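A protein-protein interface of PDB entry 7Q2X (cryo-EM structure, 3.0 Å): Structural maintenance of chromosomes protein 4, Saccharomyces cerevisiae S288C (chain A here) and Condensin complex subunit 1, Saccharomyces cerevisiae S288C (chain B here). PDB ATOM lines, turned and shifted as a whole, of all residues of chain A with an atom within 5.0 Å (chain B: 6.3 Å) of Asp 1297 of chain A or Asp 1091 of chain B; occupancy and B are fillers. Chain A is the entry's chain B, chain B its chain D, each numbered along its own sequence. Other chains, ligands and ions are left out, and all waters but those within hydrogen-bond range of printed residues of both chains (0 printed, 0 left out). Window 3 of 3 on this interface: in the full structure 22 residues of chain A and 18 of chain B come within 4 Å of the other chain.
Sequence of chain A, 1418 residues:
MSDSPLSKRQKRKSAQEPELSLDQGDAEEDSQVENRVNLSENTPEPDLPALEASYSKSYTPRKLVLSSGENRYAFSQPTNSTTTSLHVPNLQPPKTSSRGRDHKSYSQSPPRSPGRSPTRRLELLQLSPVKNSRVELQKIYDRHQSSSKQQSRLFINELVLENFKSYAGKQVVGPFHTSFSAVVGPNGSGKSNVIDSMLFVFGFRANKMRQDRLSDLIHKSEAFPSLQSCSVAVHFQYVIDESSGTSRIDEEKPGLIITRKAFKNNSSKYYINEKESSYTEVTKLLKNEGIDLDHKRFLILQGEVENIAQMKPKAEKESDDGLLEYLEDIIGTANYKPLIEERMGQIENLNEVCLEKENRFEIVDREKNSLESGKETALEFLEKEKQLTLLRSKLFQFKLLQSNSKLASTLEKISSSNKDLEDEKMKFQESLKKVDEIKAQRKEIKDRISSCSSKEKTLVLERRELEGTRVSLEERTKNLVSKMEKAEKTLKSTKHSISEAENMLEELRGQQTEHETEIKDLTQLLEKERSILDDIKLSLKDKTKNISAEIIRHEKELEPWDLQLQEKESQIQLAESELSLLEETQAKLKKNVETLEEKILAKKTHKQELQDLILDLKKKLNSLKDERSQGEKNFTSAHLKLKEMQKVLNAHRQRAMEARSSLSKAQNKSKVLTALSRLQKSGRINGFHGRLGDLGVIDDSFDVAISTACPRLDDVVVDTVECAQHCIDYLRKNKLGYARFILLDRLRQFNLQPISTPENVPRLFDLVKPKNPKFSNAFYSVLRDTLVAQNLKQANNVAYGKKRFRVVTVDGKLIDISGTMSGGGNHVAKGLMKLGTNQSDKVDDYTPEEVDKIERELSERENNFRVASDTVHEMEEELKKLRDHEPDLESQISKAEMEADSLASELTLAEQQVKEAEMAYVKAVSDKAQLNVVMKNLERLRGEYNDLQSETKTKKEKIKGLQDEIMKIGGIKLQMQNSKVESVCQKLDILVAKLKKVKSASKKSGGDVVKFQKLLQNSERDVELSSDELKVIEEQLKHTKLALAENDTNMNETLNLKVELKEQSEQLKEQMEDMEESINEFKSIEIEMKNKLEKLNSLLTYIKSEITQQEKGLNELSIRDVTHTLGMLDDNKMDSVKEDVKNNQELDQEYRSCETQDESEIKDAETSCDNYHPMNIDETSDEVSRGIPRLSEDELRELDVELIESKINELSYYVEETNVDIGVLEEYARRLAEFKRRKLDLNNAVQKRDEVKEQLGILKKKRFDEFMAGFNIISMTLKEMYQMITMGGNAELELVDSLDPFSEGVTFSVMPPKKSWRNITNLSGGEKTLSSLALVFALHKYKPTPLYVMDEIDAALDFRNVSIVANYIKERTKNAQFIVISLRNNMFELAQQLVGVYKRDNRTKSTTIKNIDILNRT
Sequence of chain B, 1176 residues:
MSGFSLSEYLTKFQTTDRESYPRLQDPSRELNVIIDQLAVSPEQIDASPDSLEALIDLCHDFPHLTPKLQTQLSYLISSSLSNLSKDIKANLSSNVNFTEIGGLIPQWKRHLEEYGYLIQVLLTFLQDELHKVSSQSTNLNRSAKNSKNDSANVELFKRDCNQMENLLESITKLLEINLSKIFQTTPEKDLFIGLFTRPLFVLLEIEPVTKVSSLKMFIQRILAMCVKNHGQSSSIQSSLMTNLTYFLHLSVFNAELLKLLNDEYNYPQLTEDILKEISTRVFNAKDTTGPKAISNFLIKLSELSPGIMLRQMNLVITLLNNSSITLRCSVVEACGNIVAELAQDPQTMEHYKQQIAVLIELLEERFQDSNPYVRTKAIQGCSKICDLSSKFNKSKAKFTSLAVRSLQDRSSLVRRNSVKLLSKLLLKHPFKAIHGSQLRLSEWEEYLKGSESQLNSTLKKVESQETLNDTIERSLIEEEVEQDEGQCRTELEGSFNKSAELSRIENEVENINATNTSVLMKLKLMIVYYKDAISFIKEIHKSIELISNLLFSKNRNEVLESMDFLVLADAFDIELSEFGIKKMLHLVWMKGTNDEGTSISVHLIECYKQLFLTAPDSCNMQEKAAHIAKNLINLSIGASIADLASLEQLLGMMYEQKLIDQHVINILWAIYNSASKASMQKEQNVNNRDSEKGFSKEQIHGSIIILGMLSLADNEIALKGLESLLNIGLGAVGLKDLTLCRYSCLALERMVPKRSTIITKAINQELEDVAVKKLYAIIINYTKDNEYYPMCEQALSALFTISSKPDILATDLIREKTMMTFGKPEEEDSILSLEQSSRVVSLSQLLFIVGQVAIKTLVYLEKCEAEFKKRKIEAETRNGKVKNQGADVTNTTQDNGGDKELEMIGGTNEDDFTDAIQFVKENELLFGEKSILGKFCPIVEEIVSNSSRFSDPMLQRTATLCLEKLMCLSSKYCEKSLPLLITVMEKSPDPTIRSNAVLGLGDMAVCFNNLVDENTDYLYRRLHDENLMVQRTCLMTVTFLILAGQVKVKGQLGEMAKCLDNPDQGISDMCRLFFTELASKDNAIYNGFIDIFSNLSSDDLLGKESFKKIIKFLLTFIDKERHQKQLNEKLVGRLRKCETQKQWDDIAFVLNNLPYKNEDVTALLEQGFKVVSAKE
NZ of Lys 1050 of chain B is in hydrogen-bond range of O of Leu 1295 of chain A, 2.8 Å away. The side-chain carboxylate (OD2) of Asp 1091 of chain B lies within hydrogen-bond range of the backbone NH (N) of Ser 1298 of chain A, at 3.1 Å. The backbone carbonyl oxygen of Val 1296 of chain A lies close to the side-chain carboxylate of Asp 1091 of chain B (2.9 Å).
The side-chain carboxylate (OD1) of Asp 1091 of chain B is in hydrogen-bond range of the side-chain hydroxyl (OG) of Ser 1094 of chain B, 3.1 Å away. OD2 of Asp 1297 of chain A lies within hydrogen-bond range of OG of Ser 1303 of chain A (3.1 Å).
CG1 of Val 1296 of chain A touches O of Asn 1087 of chain B, at 3.9 Å. Asp 1297 of chain A touches Asp 1091 of chain B (CA to OD2, 3.7 Å). Leu 1299 of chain A touches Ser 1094 of chain B.
Printed residues of chain B within 4 Å of Leu 1295 of chain A: Lys 1050. Printed residues of chain B within 4 Å of Val 1296 of chain A: Asn 1087 (3.9 Å) and Asp 1091 (2.9 Å). Of chain B, only Asp 1091 comes within 4 Å of Asp 1297 of chain A. Pro 1301 of chain A touches none of the printed residues of chain B. Gly 1054 of chain B touches none of the printed residues of chain A. Of the printed residues of chain A, Asn 1087 of chain B touches Val 1296 (3.9 Å). Of chain A, only Val 1296, Asp 1297 and Ser 1298 come within 4 Å of Asp 1091 of chain B. The nearest residue of chain B that does not touch Asp 1297 of chain A is Ser 1094 of chain B (4.2 Å). The nearest residue of chain A that does not touch Asp 1091 of chain B is Leu 1295 of chain A (4.2 Å).
Printed residues of chain B that touch a printed residue of chain A: Lys 1050, Asn 1087, Asp 1091 and Ser 1094. Of the 9 printed residues of chain A, 5 touch a printed residue of chain B. Printed residues of chain A that touch a printed residue of chain B: Leu 1295, Val 1296, Asp 1297, Ser 1298 and Leu 1299. Hydrophobic or aromatic side chains of chain A within 4 Å of the printed part of chain B: Val 1296 and Leu 1299. Among the printed residues, 6 pairs touch across the chains. Among the printed residues, no Asp or Glu carboxylate lies within 4 Å of a Lys or Arg side-chain nitrogen of the other chain.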
ATOM      1  N   LEU A1295      -0.872   9.208   3.224  1.00  0.00           N
ATOM      2  CA  LEU A1295       0.001   8.065   2.998  1.00  0.00           C
ATOM      3  C   LEU A1295       1.018   7.993   4.127  1.00  0.00           C
ATOM      4  O   LEU A1295       1.663   8.997   4.449  1.00  0.00           O
ATOM      5  CB  LEU A1295       0.721   8.171   1.649  1.00  0.00           C
ATOM      6  CG  LEU A1295      -0.012   7.728   0.378  1.00  0.00           C
ATOM      7  CD1 LEU A1295      -0.347   6.246   0.433  1.00  0.00           C
ATOM      8  CD2 LEU A1295      -1.253   8.561   0.109  1.00  0.00           C
ATOM      9  N   VAL A1296       1.153   6.811   4.730  1.00  0.00           N
ATOM     10  CA  VAL A1296       2.155   6.629   5.776  1.00  0.00           C
ATOM     11  C   VAL A1296       3.553   6.832   5.208  1.00  0.00           C
ATOM     12  O   VAL A1296       4.406   7.482   5.826  1.00  0.00           O
ATOM     13  CB  VAL A1296       1.999   5.245   6.433  1.00  0.00           C
ATOM     14  CG1 VAL A1296       3.042   5.051   7.524  1.00  0.00           C
ATOM     15  CG2 VAL A1296       0.595   5.077   6.990  1.00  0.00           C
ATOM     16  N   ASP A1297       3.809   6.284   4.023  1.00  0.00           N
ATOM     17  CA  ASP A1297       5.051   6.507   3.287  1.00  0.00           C
ATOM     18  C   ASP A1297       4.688   7.258   2.010  1.00  0.00           C
ATOM     19  O   ASP A1297       4.158   6.667   1.063  1.00  0.00           O
ATOM     20  CB  ASP A1297       5.759   5.188   2.985  1.00  0.00           C
ATOM     21  CG  ASP A1297       7.221   5.379   2.630  1.00  0.00           C
ATOM     22  OD1 ASP A1297       7.681   6.540   2.601  1.00  0.00           O
ATOM     23  OD2 ASP A1297       7.911   4.367   2.382  1.00  0.00           O
ATOM     24  N   SER A1298       4.963   8.565   1.991  1.00  0.00           N
ATOM     25  CA  SER A1298       4.577   9.388   0.849  1.00  0.00           C
ATOM     26  C   SER A1298       5.319   8.976  -0.418  1.00  0.00           C
ATOM     27  O   SER A1298       4.722   8.901  -1.497  1.00  0.00           O
ATOM     28  CB  SER A1298       4.825  10.864   1.160  1.00  0.00           C
ATOM     29  OG  SER A1298       4.146  11.701   0.240  1.00  0.00           O
ATOM     30  N   LEU A1299       6.623   8.709  -0.308  1.00  0.00           N
ATOM     31  CA  LEU A1299       7.403   8.349  -1.487  1.00  0.00           C
ATOM     32  C   LEU A1299       7.074   6.946  -1.981  1.00  0.00           C
ATOM     33  O   LEU A1299       7.234   6.656  -3.172  1.00  0.00           O
ATOM     34  CB  LEU A1299       8.900   8.471  -1.193  1.00  0.00           C
ATOM     35  CG  LEU A1299       9.556   9.852  -1.326  1.00  0.00           C
ATOM     36  CD1 LEU A1299       9.493  10.334  -2.769  1.00  0.00           C
ATOM     37  CD2 LEU A1299       8.943  10.883  -0.387  1.00  0.00           C
ATOM     38  N   ASP A1300       6.614   6.066  -1.094  1.00  0.00           N
ATOM     39  CA  ASP A1300       6.251   4.692  -1.443  1.00  0.00           C
ATOM     40  C   ASP A1300       4.829   4.442  -0.963  1.00  0.00           C
ATOM     41  O   ASP A1300       4.614   3.895   0.128  1.00  0.00           O
ATOM     42  CB  ASP A1300       7.234   3.687  -0.838  1.00  0.00           C
ATOM     43  CG  ASP A1300       7.375   2.434  -1.679  1.00  0.00           C
ATOM     44  OD1 ASP A1300       6.614   2.284  -2.658  1.00  0.00           O
ATOM     45  OD2 ASP A1300       8.246   1.597  -1.360  1.00  0.00           O
ATOM     46  N   PRO A1301       3.828   4.848  -1.751  1.00  0.00           N
ATOM     47  CA  PRO A1301       2.433   4.694  -1.300  1.00  0.00           C
ATOM     48  C   PRO A1301       2.029   3.255  -1.023  1.00  0.00           C
ATOM     49  O   PRO A1301       1.236   3.006  -0.106  1.00  0.00           O
ATOM     50  CB  PRO A1301       1.625   5.293  -2.461  1.00  0.00           C
ATOM     51  CG  PRO A1301       2.585   6.177  -3.186  1.00  0.00           C
ATOM     52  CD  PRO A1301       3.919   5.513  -3.060  1.00  0.00           C
ATOM     53  N   SER A1303       3.975   0.782  -0.011  1.00  0.00           N
ATOM     54  CA  SER A1303       4.792   0.095   0.982  1.00  0.00           C
ATOM     55  C   SER A1303       4.080  -0.020   2.325  1.00  0.00           C
ATOM     56  O   SER A1303       4.209  -1.039   3.012  1.00  0.00           O
ATOM     57  CB  SER A1303       6.129   0.817   1.154  1.00  0.00           C
ATOM     58  OG  SER A1303       5.947   2.092   1.742  1.00  0.00           O
ATOM     59  N   GLU A1304       3.328   1.009   2.716  1.00  0.00           N
ATOM     60  CA  GLU A1304       2.699   1.046   4.033  1.00  0.00           C
ATOM     61  C   GLU A1304       1.180   0.989   3.952  1.00  0.00           C
ATOM     62  O   GLU A1304       0.569   0.122   4.586  1.00  0.00           O
ATOM     63  CB  GLU A1304       3.155   2.298   4.791  1.00  0.00           C
ATOM     64  N   LYS B1050       2.259  14.531  11.535  1.00  0.00           N
ATOM     65  CA  LYS B1050       2.917  13.677  10.549  1.00  0.00           C
ATOM     66  C   LYS B1050       3.454  14.484   9.371  1.00  0.00           C
ATOM     67  O   LYS B1050       4.571  14.237   8.900  1.00  0.00           O
ATOM     68  CB  LYS B1050       1.946  12.602  10.060  1.00  0.00           C
ATOM     69  CG  LYS B1050       2.555  11.610   9.082  1.00  0.00           C
ATOM     70  CD  LYS B1050       1.479  10.872   8.303  1.00  0.00           C
ATOM     71  CE  LYS B1050       1.005  11.685   7.109  1.00  0.00           C
ATOM     72  NZ  LYS B1050       1.839  11.435   5.901  1.00  0.00           N
ATOM     73  N   GLY B1054       9.944  16.325   7.420  1.00  0.00           N
ATOM     74  CA  GLY B1054      11.247  16.462   6.788  1.00  0.00           C
ATOM     75  C   GLY B1054      11.786  17.877   6.859  1.00  0.00           C
ATOM     76  O   GLY B1054      12.974  18.087   7.118  1.00  0.00           O
ATOM     77  N   TYR B1086       8.434   8.018  14.842  1.00  0.00           N
ATOM     78  CA  TYR B1086       8.587   6.675  14.292  1.00  0.00           C
ATOM     79  C   TYR B1086       7.661   6.472  13.099  1.00  0.00           C
ATOM     80  O   TYR B1086       8.093   6.013  12.034  1.00  0.00           O
ATOM     81  CB  TYR B1086       8.316   5.630  15.375  1.00  0.00           C
ATOM     82  CG  TYR B1086       8.263   4.207  14.862  1.00  0.00           C
ATOM     83  CD1 TYR B1086       9.429   3.488  14.635  1.00  0.00           C
ATOM     84  CD2 TYR B1086       7.049   3.581  14.612  1.00  0.00           C
ATOM     85  CE1 TYR B1086       9.387   2.187  14.167  1.00  0.00           C
ATOM     86  CE2 TYR B1086       6.996   2.282  14.145  1.00  0.00           C
ATOM     87  CZ  TYR B1086       8.168   1.589  13.924  1.00  0.00           C
ATOM     88  OH  TYR B1086       8.121   0.295  13.459  1.00  0.00           O
ATOM     89  N   ASN B1087       6.391   6.863  13.244  1.00  0.00           N
ATOM     90  CA  ASN B1087       5.428   6.689  12.163  1.00  0.00           C
ATOM     91  C   ASN B1087       5.822   7.462  10.914  1.00  0.00           C
ATOM     92  O   ASN B1087       5.336   7.146   9.822  1.00  0.00           O
ATOM     93  CB  ASN B1087       4.035   7.118  12.624  1.00  0.00           C
ATOM     94  CG  ASN B1087       3.354   6.065  13.476  1.00  0.00           C
ATOM     95  OD1 ASN B1087       3.363   4.880  13.143  1.00  0.00           O
ATOM     96  ND2 ASN B1087       2.758   6.493  14.583  1.00  0.00           N
ATOM     97  N   GLY B1088       6.686   8.465  11.045  1.00  0.00           N
ATOM     98  CA  GLY B1088       7.168   9.193   9.892  1.00  0.00           C
ATOM     99  C   GLY B1088       8.661   9.049   9.689  1.00  0.00           C
ATOM    100  O   GLY B1088       9.223   9.661   8.775  1.00  0.00           O
ATOM    101  N   PHE B1089       9.308   8.233  10.530  1.00  0.00           N
ATOM    102  CA  PHE B1089      10.765   8.135  10.515  1.00  0.00           C
ATOM    103  C   PHE B1089      11.288   7.826   9.118  1.00  0.00           C
ATOM    104  O   PHE B1089      12.053   8.606   8.538  1.00  0.00           O
ATOM    105  CB  PHE B1089      11.229   7.070  11.511  1.00  0.00           C
ATOM    106  CG  PHE B1089      12.721   7.013  11.687  1.00  0.00           C
ATOM    107  CD1 PHE B1089      13.353   7.833  12.606  1.00  0.00           C
ATOM    108  CD2 PHE B1089      13.489   6.144  10.931  1.00  0.00           C
ATOM    109  CE1 PHE B1089      14.724   7.787  12.769  1.00  0.00           C
ATOM    110  CE2 PHE B1089      14.861   6.093  11.089  1.00  0.00           C
ATOM    111  CZ  PHE B1089      15.479   6.915  12.010  1.00  0.00           C
ATOM    112  N   ILE B1090      10.858   6.696   8.553  1.00  0.00           N
ATOM    113  CA  ILE B1090      11.261   6.348   7.194  1.00  0.00           C
ATOM    114  C   ILE B1090      10.860   7.453   6.227  1.00  0.00           C
ATOM    115  O   ILE B1090      11.636   7.835   5.342  1.00  0.00           O
ATOM    116  CB  ILE B1090      10.664   4.987   6.789  1.00  0.00           C
ATOM    117  CG1 ILE B1090       9.184   4.913   7.170  1.00  0.00           C
ATOM    118  CG2 ILE B1090      11.433   3.856   7.449  1.00  0.00           C
ATOM    119  CD1 ILE B1090       8.471   3.700   6.612  1.00  0.00           C
ATOM    120  N   ASP B1091       9.657   8.007   6.405  1.00  0.00           N
ATOM    121  CA  ASP B1091       9.225   9.126   5.576  1.00  0.00           C
ATOM    122  C   ASP B1091      10.212  10.281   5.676  1.00  0.00           C
ATOM    123  O   ASP B1091      10.599  10.871   4.659  1.00  0.00           O
ATOM    124  CB  ASP B1091       7.822   9.574   5.987  1.00  0.00           C
ATOM    125  CG  ASP B1091       7.015  10.105   4.818  1.00  0.00           C
ATOM    126  OD1 ASP B1091       7.581  10.855   3.995  1.00  0.00           O
ATOM    127  OD2 ASP B1091       5.814   9.775   4.723  1.00  0.00           O
ATOM    128  N   ILE B1092      10.654  10.598   6.897  1.00  0.00           N
ATOM    129  CA  ILE B1092      11.686  11.616   7.066  1.00  0.00           C
ATOM    130  C   ILE B1092      12.921  11.240   6.260  1.00  0.00           C
ATOM    131  O   ILE B1092      13.458  12.052   5.494  1.00  0.00           O
ATOM    132  CB  ILE B1092      12.019  11.806   8.557  1.00  0.00           C
ATOM    133  CG1 ILE B1092      10.822  12.399   9.302  1.00  0.00           C
ATOM    134  CG2 ILE B1092      13.244  12.692   8.721  1.00  0.00           C
ATOM    135  CD1 ILE B1092      10.743  11.989  10.755  1.00  0.00           C
ATOM    136  N   PHE B1093      13.357   9.982   6.382  1.00  0.00           N
ATOM    137  CA  PHE B1093      14.473   9.513   5.572  1.00  0.00           C
ATOM    138  C   PHE B1093      14.153   9.648   4.091  1.00  0.00           C
ATOM    139  O   PHE B1093      15.007  10.066   3.298  1.00  0.00           O
ATOM    140  CB  PHE B1093      14.809   8.064   5.922  1.00  0.00           C
ATOM    141  CG  PHE B1093      15.895   7.473   5.071  1.00  0.00           C
ATOM    142  CD1 PHE B1093      17.203   7.912   5.189  1.00  0.00           C
ATOM    143  CD2 PHE B1093      15.608   6.479   4.149  1.00  0.00           C
ATOM    144  CE1 PHE B1093      18.205   7.371   4.407  1.00  0.00           C
ATOM    145  CE2 PHE B1093      16.605   5.935   3.362  1.00  0.00           C
ATOM    146  CZ  PHE B1093      17.905   6.382   3.492  1.00  0.00           C
ATOM    147  N   SER B1094      12.912   9.330   3.707  1.00  0.00           N
ATOM    148  CA  SER B1094      12.498   9.522   2.323  1.00  0.00           C
ATOM    149  C   SER B1094      12.687  10.971   1.899  1.00  0.00           C
ATOM    150  O   SER B1094      13.190  11.245   0.802  1.00  0.00           O
ATOM    151  CB  SER B1094      11.043   9.090   2.145  1.00  0.00           C
ATOM    152  OG  SER B1094      10.156  10.129   2.520  1.00  0.00           O
ATOM    153  N   ASN B1095      12.326  11.915   2.776  1.00  0.00           N
ATOM    154  CA  ASN B1095      12.545  13.323   2.466  1.00  0.00           C
ATOM    155  C   ASN B1095      14.020  13.596   2.217  1.00  0.00           C
ATOM    156  O   ASN B1095      14.376  14.326   1.283  1.00  0.00           O
ATOM    157  CB  ASN B1095      12.014  14.201   3.599  1.00  0.00           C
ATOM    158  CG  ASN B1095      11.620  15.586   3.126  1.00  0.00           C
ATOM    159  OD1 ASN B1095      12.363  16.240   2.394  1.00  0.00           O
ATOM    160  ND2 ASN B1095      10.443  16.040   3.541  1.00  0.00           N
ATOM    161  N   LEU B1096      14.896  12.989   3.023  1.00  0.00           N
ATOM    162  CA  LEU B1096      16.326  13.120   2.779  1.00  0.00           C
ATOM    163  C   LEU B1096      16.691  12.566   1.409  1.00  0.00           C
ATOM    164  O   LEU B1096      17.460  13.185   0.663  1.00  0.00           O
ATOM    165  CB  LEU B1096      17.112  12.412   3.883  1.00  0.00           C
ATOM    166  CG  LEU B1096      16.738  12.816   5.311  1.00  0.00           C
ATOM    167  CD1 LEU B1096      17.299  11.829   6.324  1.00  0.00           C
ATOM    168  CD2 LEU B1096      17.217  14.228   5.611  1.00  0.00           C
ATOM    169  N   ARG B1134      14.514  -2.708   2.654  1.00  0.00           N
ATOM    170  CA  ARG B1134      14.944  -1.634   1.763  1.00  0.00           C
ATOM    171  C   ARG B1134      16.309  -1.919   1.147  1.00  0.00           C
ATOM    172  O   ARG B1134      16.611  -1.419   0.058  1.00  0.00           O
ATOM    173  CB  ARG B1134      14.973  -0.305   2.517  1.00  0.00           C
ATOM    174  CG  ARG B1134      13.606   0.327   2.713  1.00  0.00           C
ATOM    175  CD  ARG B1134      13.729   1.725   3.294  1.00  0.00           C
ATOM    176  NE  ARG B1134      14.107   1.695   4.701  1.00  0.00           N
ATOM    177  CZ  ARG B1134      13.270   1.437   5.697  1.00  0.00           C
ATOM    178  NH1 ARG B1134      11.990   1.183   5.477  1.00  0.00           N
ATOM    179  NH2 ARG B1134      13.729   1.431   6.945  1.00  0.00           N
